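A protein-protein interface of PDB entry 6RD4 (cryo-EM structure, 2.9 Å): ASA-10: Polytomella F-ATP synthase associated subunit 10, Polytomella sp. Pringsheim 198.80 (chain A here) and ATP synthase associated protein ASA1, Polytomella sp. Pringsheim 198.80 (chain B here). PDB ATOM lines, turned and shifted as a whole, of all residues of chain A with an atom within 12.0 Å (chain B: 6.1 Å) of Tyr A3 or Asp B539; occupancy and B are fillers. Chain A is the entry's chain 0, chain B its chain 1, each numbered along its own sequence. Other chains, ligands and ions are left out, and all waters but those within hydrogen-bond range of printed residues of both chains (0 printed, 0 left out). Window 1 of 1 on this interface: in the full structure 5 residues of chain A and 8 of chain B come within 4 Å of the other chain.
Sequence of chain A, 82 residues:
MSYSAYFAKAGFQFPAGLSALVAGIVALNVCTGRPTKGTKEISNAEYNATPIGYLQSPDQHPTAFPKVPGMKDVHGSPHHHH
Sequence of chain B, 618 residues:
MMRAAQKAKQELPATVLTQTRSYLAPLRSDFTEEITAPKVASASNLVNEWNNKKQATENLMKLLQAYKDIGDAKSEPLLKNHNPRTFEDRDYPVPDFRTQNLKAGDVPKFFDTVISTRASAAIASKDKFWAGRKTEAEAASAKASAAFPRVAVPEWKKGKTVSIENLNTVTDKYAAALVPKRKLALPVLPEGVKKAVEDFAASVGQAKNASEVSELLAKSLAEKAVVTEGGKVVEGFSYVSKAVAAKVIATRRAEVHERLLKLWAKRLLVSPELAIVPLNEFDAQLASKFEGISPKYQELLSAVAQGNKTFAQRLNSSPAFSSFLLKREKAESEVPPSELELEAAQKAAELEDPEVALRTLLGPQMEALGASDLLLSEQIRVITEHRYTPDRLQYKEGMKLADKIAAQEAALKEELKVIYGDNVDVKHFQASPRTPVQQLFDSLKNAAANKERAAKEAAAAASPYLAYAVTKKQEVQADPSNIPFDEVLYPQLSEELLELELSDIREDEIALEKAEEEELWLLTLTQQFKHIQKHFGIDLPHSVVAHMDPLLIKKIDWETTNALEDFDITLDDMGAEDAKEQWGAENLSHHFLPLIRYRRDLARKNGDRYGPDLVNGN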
ATOM      1  N   SER A   2      -2.685   5.456 -10.424  1.00  0.00           N
ATOM      2  CA  SER A   2      -1.853   5.762  -9.286  1.00  0.00           C
ATOM      3  C   SER A   2      -2.443   5.061  -8.107  1.00  0.00           C
ATOM      4  O   SER A   2      -3.325   5.592  -7.465  1.00  0.00           O
ATOM      5  CB  SER A   2      -1.769   7.264  -9.060  1.00  0.00           C
ATOM      6  OG  SER A   2      -0.904   7.869 -10.004  1.00  0.00           O
ATOM      7  N   TYR A   3      -2.014   3.814  -7.913  1.00  0.00           N
ATOM      8  CA  TYR A   3      -2.338   2.909  -6.810  1.00  0.00           C
ATOM      9  C   TYR A   3      -3.786   2.455  -6.777  1.00  0.00           C
ATOM     10  O   TYR A   3      -4.119   1.607  -5.964  1.00  0.00           O
ATOM     11  CB  TYR A   3      -2.003   3.512  -5.447  1.00  0.00           C
ATOM     12  CG  TYR A   3      -0.551   3.596  -5.135  1.00  0.00           C
ATOM     13  CD1 TYR A   3       0.297   2.589  -5.484  1.00  0.00           C
ATOM     14  CD2 TYR A   3      -0.034   4.694  -4.490  1.00  0.00           C
ATOM     15  CE1 TYR A   3       1.612   2.682  -5.221  1.00  0.00           C
ATOM     16  CE2 TYR A   3       1.277   4.781  -4.219  1.00  0.00           C
ATOM     17  CZ  TYR A   3       2.093   3.773  -4.592  1.00  0.00           C
ATOM     18  OH  TYR A   3       3.428   3.830  -4.344  1.00  0.00           O
ATOM     19  N   SER A   4      -4.655   2.975  -7.638  1.00  0.00           N
ATOM     20  CA  SER A   4      -6.027   2.491  -7.659  1.00  0.00           C
ATOM     21  C   SER A   4      -6.111   1.112  -8.265  1.00  0.00           C
ATOM     22  O   SER A   4      -6.950   0.312  -7.867  1.00  0.00           O
ATOM     23  CB  SER A   4      -6.925   3.433  -8.443  1.00  0.00           C
ATOM     24  OG  SER A   4      -7.154   4.630  -7.745  1.00  0.00           O
ATOM     25  N   ALA A   5      -5.252   0.817  -9.219  1.00  0.00           N
ATOM     26  CA  ALA A   5      -5.228  -0.471  -9.875  1.00  0.00           C
ATOM     27  C   ALA A   5      -4.439  -1.513  -9.114  1.00  0.00           C
ATOM     28  O   ALA A   5      -4.418  -2.668  -9.530  1.00  0.00           O
ATOM     29  CB  ALA A   5      -4.638  -0.309 -11.261  1.00  0.00           C
ATOM     30  N   TYR A   6      -3.756  -1.132  -8.048  1.00  0.00           N
ATOM     31  CA  TYR A   6      -3.105  -2.111  -7.199  1.00  0.00           C
ATOM     32  C   TYR A   6      -4.087  -2.717  -6.221  1.00  0.00           C
ATOM     33  O   TYR A   6      -3.948  -3.878  -5.835  1.00  0.00           O
ATOM     34  CB  TYR A   6      -1.948  -1.450  -6.463  1.00  0.00           C
ATOM     35  CG  TYR A   6      -1.365  -2.264  -5.364  1.00  0.00           C
ATOM     36  CD1 TYR A   6      -0.705  -3.430  -5.632  1.00  0.00           C
ATOM     37  CD2 TYR A   6      -1.481  -1.870  -4.063  1.00  0.00           C
ATOM     38  CE1 TYR A   6      -0.179  -4.179  -4.628  1.00  0.00           C
ATOM     39  CE2 TYR A   6      -0.958  -2.605  -3.058  1.00  0.00           C
ATOM     40  CZ  TYR A   6      -0.310  -3.759  -3.341  1.00  0.00           C
ATOM     41  OH  TYR A   6       0.218  -4.511  -2.331  1.00  0.00           O
ATOM     42  N   PHE A   7      -5.087  -1.950  -5.825  1.00  0.00           N
ATOM     43  CA  PHE A   7      -6.089  -2.401  -4.887  1.00  0.00           C
ATOM     44  C   PHE A   7      -7.255  -3.089  -5.552  1.00  0.00           C
ATOM     45  O   PHE A   7      -8.064  -3.703  -4.855  1.00  0.00           O
ATOM     46  CB  PHE A   7      -6.583  -1.228  -4.068  1.00  0.00           C
ATOM     47  CG  PHE A   7      -5.566  -0.705  -3.153  1.00  0.00           C
ATOM     48  CD1 PHE A   7      -4.939  -1.546  -2.266  1.00  0.00           C
ATOM     49  CD2 PHE A   7      -5.207   0.604  -3.191  1.00  0.00           C
ATOM     50  CE1 PHE A   7      -3.993  -1.075  -1.443  1.00  0.00           C
ATOM     51  CE2 PHE A   7      -4.258   1.069  -2.368  1.00  0.00           C
ATOM     52  CZ  PHE A   7      -3.655   0.229  -1.498  1.00  0.00           C
ATOM     53  N   ALA A   8      -7.366  -3.005  -6.864  1.00  0.00           N
ATOM     54  CA  ALA A   8      -8.354  -3.802  -7.560  1.00  0.00           C
ATOM     55  C   ALA A   8      -7.862  -5.206  -7.851  1.00  0.00           C
ATOM     56  O   ALA A   8      -8.672  -6.062  -8.201  1.00  0.00           O
ATOM     57  CB  ALA A   8      -8.754  -3.108  -8.853  1.00  0.00           C
ATOM     58  N   LYS A   9      -6.566  -5.463  -7.708  1.00  0.00           N
ATOM     59  CA  LYS A   9      -6.003  -6.760  -8.055  1.00  0.00           C
ATOM     60  C   LYS A   9      -6.366  -7.821  -7.036  1.00  0.00           C
ATOM     61  O   LYS A   9      -6.848  -8.896  -7.395  1.00  0.00           O
ATOM     62  CB  LYS A   9      -4.490  -6.664  -8.183  1.00  0.00           C
ATOM     63  CG  LYS A   9      -4.057  -5.939  -9.411  1.00  0.00           C
ATOM     64  CD  LYS A   9      -2.570  -5.761  -9.424  1.00  0.00           C
ATOM     65  CE  LYS A   9      -2.160  -4.914 -10.592  1.00  0.00           C
ATOM     66  NZ  LYS A   9      -0.714  -5.049 -10.836  1.00  0.00           N
ATOM     67  N   ALA A  10      -6.096  -7.565  -5.769  1.00  0.00           N
ATOM     68  CA  ALA A  10      -6.572  -8.460  -4.728  1.00  0.00           C
ATOM     69  C   ALA A  10      -8.057  -8.224  -4.542  1.00  0.00           C
ATOM     70  O   ALA A  10      -8.481  -7.104  -4.257  1.00  0.00           O
ATOM     71  CB  ALA A  10      -5.813  -8.228  -3.428  1.00  0.00           C
ATOM     72  N   GLY A  11      -8.853  -9.259  -4.745  1.00  0.00           N
ATOM     73  CA  GLY A  11     -10.282  -9.069  -4.755  1.00  0.00           C
ATOM     74  C   GLY A  11     -10.883  -9.109  -3.374  1.00  0.00           C
ATOM     75  O   GLY A  11     -10.404  -8.433  -2.466  1.00  0.00           O
ATOM     76  N   ARG B 314      -7.627  14.050  -6.951  1.00  0.00           N
ATOM     77  CA  ARG B 314      -6.958  12.811  -6.590  1.00  0.00           C
ATOM     78  C   ARG B 314      -7.875  11.886  -5.825  1.00  0.00           C
ATOM     79  O   ARG B 314      -7.647  10.678  -5.820  1.00  0.00           O
ATOM     80  CB  ARG B 314      -5.719  13.088  -5.750  1.00  0.00           C
ATOM     81  CG  ARG B 314      -4.598  13.699  -6.490  1.00  0.00           C
ATOM     82  CD  ARG B 314      -3.346  13.661  -5.687  1.00  0.00           C
ATOM     83  NE  ARG B 314      -3.554  14.140  -4.335  1.00  0.00           N
ATOM     84  CZ  ARG B 314      -3.227  15.348  -3.915  1.00  0.00           C
ATOM     85  NH1 ARG B 314      -2.671  16.207  -4.738  1.00  0.00           N
ATOM     86  NH2 ARG B 314      -3.438  15.696  -2.665  1.00  0.00           N
ATOM     87  N   SER B 317     -10.175   9.735  -8.443  1.00  0.00           N
ATOM     88  CA  SER B 317      -9.541   8.556  -8.989  1.00  0.00           C
ATOM     89  C   SER B 317      -9.084   7.598  -7.908  1.00  0.00           C
ATOM     90  O   SER B 317      -8.327   6.668  -8.197  1.00  0.00           O
ATOM     91  CB  SER B 317      -8.372   8.968  -9.866  1.00  0.00           C
ATOM     92  OG  SER B 317      -7.396   9.620  -9.092  1.00  0.00           O
ATOM     93  N   SER B 318      -9.516   7.818  -6.670  1.00  0.00           N
ATOM     94  CA  SER B 318      -9.272   6.910  -5.571  1.00  0.00           C
ATOM     95  C   SER B 318     -10.056   5.627  -5.789  1.00  0.00           C
ATOM     96  O   SER B 318     -11.017   5.610  -6.556  1.00  0.00           O
ATOM     97  CB  SER B 318      -9.708   7.563  -4.269  1.00  0.00           C
ATOM     98  OG  SER B 318      -9.222   6.901  -3.130  1.00  0.00           O
ATOM     99  N   PRO B 319      -9.673   4.534  -5.126  1.00  0.00           N
ATOM    100  CA  PRO B 319     -10.519   3.340  -5.161  1.00  0.00           C
ATOM    101  C   PRO B 319     -11.858   3.512  -4.487  1.00  0.00           C
ATOM    102  O   PRO B 319     -12.737   2.677  -4.683  1.00  0.00           O
ATOM    103  CB  PRO B 319      -9.668   2.300  -4.443  1.00  0.00           C
ATOM    104  CG  PRO B 319      -8.323   2.736  -4.637  1.00  0.00           C
ATOM    105  CD  PRO B 319      -8.327   4.205  -4.645  1.00  0.00           C
ATOM    106  N   HIS B 531       5.851  11.994  -1.486  1.00  0.00           N
ATOM    107  CA  HIS B 531       5.063  10.882  -1.965  1.00  0.00           C
ATOM    108  C   HIS B 531       4.072  10.400  -0.937  1.00  0.00           C
ATOM    109  O   HIS B 531       2.997   9.939  -1.305  1.00  0.00           O
ATOM    110  CB  HIS B 531       5.965   9.739  -2.366  1.00  0.00           C
ATOM    111  CG  HIS B 531       5.248   8.640  -3.063  1.00  0.00           C
ATOM    112  ND1 HIS B 531       5.095   7.395  -2.514  1.00  0.00           N
ATOM    113  CD2 HIS B 531       4.608   8.609  -4.248  1.00  0.00           C
ATOM    114  CE1 HIS B 531       4.416   6.633  -3.343  1.00  0.00           C
ATOM    115  NE2 HIS B 531       4.109   7.346  -4.406  1.00  0.00           N
ATOM    116  N   LYS B 534       1.256  13.222  -0.999  1.00  0.00           N
ATOM    117  CA  LYS B 534       0.439  13.182  -2.197  1.00  0.00           C
ATOM    118  C   LYS B 534      -0.589  12.073  -2.131  1.00  0.00           C
ATOM    119  O   LYS B 534      -1.658  12.184  -2.729  1.00  0.00           O
ATOM    120  CB  LYS B 534       1.359  12.995  -3.390  1.00  0.00           C
ATOM    121  CG  LYS B 534       0.754  13.122  -4.731  1.00  0.00           C
ATOM    122  CD  LYS B 534       1.725  12.660  -5.756  1.00  0.00           C
ATOM    123  CE  LYS B 534       1.044  12.501  -7.071  1.00  0.00           C
ATOM    124  NZ  LYS B 534       1.967  11.905  -8.079  1.00  0.00           N
ATOM    125  N   HIS B 535      -0.297  11.011  -1.397  1.00  0.00           N
ATOM    126  CA  HIS B 535      -1.061   9.784  -1.445  1.00  0.00           C
ATOM    127  C   HIS B 535      -1.638   9.340  -0.118  1.00  0.00           C
ATOM    128  O   HIS B 535      -2.422   8.400  -0.119  1.00  0.00           O
ATOM    129  CB  HIS B 535      -0.189   8.646  -1.979  1.00  0.00           C
ATOM    130  CG  HIS B 535       0.061   8.706  -3.447  1.00  0.00           C
ATOM    131  ND1 HIS B 535      -0.922   8.466  -4.375  1.00  0.00           N
ATOM    132  CD2 HIS B 535       1.184   8.952  -4.150  1.00  0.00           C
ATOM    133  CE1 HIS B 535      -0.421   8.587  -5.586  1.00  0.00           C
ATOM    134  NE2 HIS B 535       0.856   8.880  -5.476  1.00  0.00           N
ATOM    135  N   PHE B 536      -1.264   9.940   1.004  1.00  0.00           N
ATOM    136  CA  PHE B 536      -1.747   9.476   2.295  1.00  0.00           C
ATOM    137  C   PHE B 536      -3.204   9.826   2.463  1.00  0.00           C
ATOM    138  O   PHE B 536      -3.602  10.968   2.238  1.00  0.00           O
ATOM    139  CB  PHE B 536      -0.955  10.108   3.425  1.00  0.00           C
ATOM    140  CG  PHE B 536      -1.219   9.515   4.743  1.00  0.00           C
ATOM    141  CD1 PHE B 536      -0.697   8.302   5.074  1.00  0.00           C
ATOM    142  CD2 PHE B 536      -1.987  10.173   5.657  1.00  0.00           C
ATOM    143  CE1 PHE B 536      -0.947   7.765   6.270  1.00  0.00           C
ATOM    144  CE2 PHE B 536      -2.231   9.630   6.841  1.00  0.00           C
ATOM    145  CZ  PHE B 536      -1.711   8.428   7.153  1.00  0.00           C
ATOM    146  N   GLY B 537      -4.000   8.852   2.878  1.00  0.00           N
ATOM    147  CA  GLY B 537      -5.405   9.069   3.053  1.00  0.00           C
ATOM    148  C   GLY B 537      -6.190   9.063   1.774  1.00  0.00           C
ATOM    149  O   GLY B 537      -7.383   9.365   1.799  1.00  0.00           O
ATOM    150  N   ILE B 538      -5.559   8.748   0.656  1.00  0.00           N
ATOM    151  CA  ILE B 538      -6.248   8.633  -0.614  1.00  0.00           C
ATOM    152  C   ILE B 538      -6.024   7.233  -1.143  1.00  0.00           C
ATOM    153  O   ILE B 538      -6.957   6.436  -1.190  1.00  0.00           O
ATOM    154  CB  ILE B 538      -5.768   9.694  -1.615  1.00  0.00           C
ATOM    155  CG1 ILE B 538      -6.156  11.077  -1.147  1.00  0.00           C
ATOM    156  CG2 ILE B 538      -6.388   9.483  -2.924  1.00  0.00           C
ATOM    157  CD1 ILE B 538      -5.331  12.129  -1.721  1.00  0.00           C
ATOM    158  N   ASP B 539      -4.800   6.896  -1.514  1.00  0.00           N
ATOM    159  CA  ASP B 539      -4.585   5.560  -2.043  1.00  0.00           C
ATOM    160  C   ASP B 539      -3.262   4.927  -1.661  1.00  0.00           C
ATOM    161  O   ASP B 539      -2.880   3.956  -2.302  1.00  0.00           O
ATOM    162  CB  ASP B 539      -4.715   5.525  -3.568  1.00  0.00           C
ATOM    163  CG  ASP B 539      -3.999   6.669  -4.264  1.00  0.00           C
ATOM    164  OD1 ASP B 539      -2.955   7.126  -3.791  1.00  0.00           O
ATOM    165  OD2 ASP B 539      -4.479   7.117  -5.316  1.00  0.00           O
ATOM    166  N   LEU B 540      -2.544   5.432  -0.686  1.00  0.00           N
ATOM    167  CA  LEU B 540      -1.227   4.886  -0.403  1.00  0.00           C
ATOM    168  C   LEU B 540      -1.382   3.558   0.305  1.00  0.00           C
ATOM    169  O   LEU B 540      -2.132   3.478   1.265  1.00  0.00           O
ATOM    170  CB  LEU B 540      -0.440   5.841   0.471  1.00  0.00           C
ATOM    171  CG  LEU B 540       1.031   5.710   0.835  1.00  0.00           C
ATOM    172  CD1 LEU B 540       1.883   5.733  -0.340  1.00  0.00           C
ATOM    173  CD2 LEU B 540       1.349   6.845   1.673  1.00  0.00           C
ATOM    174  N   PRO B 541      -0.740   2.497  -0.146  1.00  0.00           N
ATOM    175  CA  PRO B 541      -0.809   1.261   0.605  1.00  0.00           C
ATOM    176  C   PRO B 541       0.044   1.328   1.848  1.00  0.00           C
ATOM    177  O   PRO B 541       0.948   2.140   1.977  1.00  0.00           O
ATOM    178  CB  PRO B 541      -0.287   0.220  -0.381  1.00  0.00           C
ATOM    179  CG  PRO B 541       0.323   0.911  -1.386  1.00  0.00           C
ATOM    180  CD  PRO B 541      -0.233   2.245  -1.489  1.00  0.00           C
ATOM    181  N   VAL B 544       3.836   0.450   1.226  1.00  0.00           N
ATOM    182  CA  VAL B 544       4.716   1.468   0.690  1.00  0.00           C
ATOM    183  C   VAL B 544       5.171   2.394   1.787  1.00  0.00           C
ATOM    184  O   VAL B 544       6.310   2.852   1.778  1.00  0.00           O
ATOM    185  CB  VAL B 544       3.994   2.189  -0.454  1.00  0.00           C
ATOM    186  CG1 VAL B 544       4.714   3.376  -0.905  1.00  0.00           C
ATOM    187  CG2 VAL B 544       3.928   1.281  -1.590  1.00  0.00           C
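The backbone carbonyl oxygen (O) of Ser A2 sits close to the side-chain carboxylate (OD2) of Asp B539, 2.9 Å away.
OG of Ser A4 lies close to O of Ser B317, 2.4 Å away.
The side-chain hydroxyl (OG) of Ser B317 sits at hydrogen-bond distance from the backbone carbonyl oxygen (O) of Arg B314, at 3.4 Å.
O of Ile B538 is in hydrogen-bond range of OG of Ser B318 (3.0 Å).
OD1 of Asp B539 sits at hydrogen-bond distance from ND1 of His B535 (2.5 Å).
The backbone NH of Leu B540 lies within hydrogen-bond range of the backbone carbonyl oxygen of His B535.
Among the printed residues, merely in contact across the chains: Ser A2 with His B535, Tyr A3 with His B531, Tyr A3 with His B535, Tyr A3 with Asp B539, Tyr A3 with Pro B541, Tyr A3 with Val B544, Ser A4 with Ser B318, Ser A4 with Pro B319, Tyr A6 with Pro B541, Phe A7 with Asp B539 and Phe A7 with Pro B541.
Of the printed residues of chain B, Ser A2 touches His B535 (3.95 Å) and Asp B539 (2.9 Å).
Of chain B, only His B531, His B535, Asp B539, Pro B541 and Val B544 come within 4 Å of Tyr A3.
Of the printed residues of chain B, Ser A4 touches Ser B317, Ser B318 and Pro B319.
Ala A5 touches none of the printed residues of chain B.
Printed residues of chain B within 4 Å of Tyr A6: Pro B541 (3.9 Å).
Of the printed residues of chain B, Phe A7 touches Asp B539 and Pro B541.
Of chain A, only Ser A4 comes within 4 Å of Ser B317.
Of the printed residues of chain A, Ser B318 touches Ser A4 (3.6 Å).
Of the printed residues of chain A, His B531 touches Tyr A3 (3.1 Å).
His B535 touches just these residues of chain A: Ser A2 and Tyr A3.
No residue of chain A comes within 4 Å of Gly B537.
Asp B539 touches just these residues of chain A: Ser A2, Tyr A3 and Phe A7.
No residue of chain A comes within 4 Å of Leu B540.
Of chain A, only Tyr A3 comes within 4 Å of Val B544.
The nearest residue of chain B that does not touch Tyr A3 is Leu B540 (4.04 Å).
The nearest residue of chain A that does not touch Asp B539 is Ser A4 (4.4 Å).
Hydrophobic or aromatic side chains of chain A within 4 Å of the printed part of chain B: Tyr A3, Tyr A6 and Phe A7.
Hydrophobic or aromatic side chains of chain B within 4 Å of the printed part of chain A: Pro B319, His B531, His B535, Pro B541 and Val B544.
Among the printed residues, no Asp or Glu carboxylate lies within 4 Å of a Lys or Arg side-chain nitrogen of the other chain.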
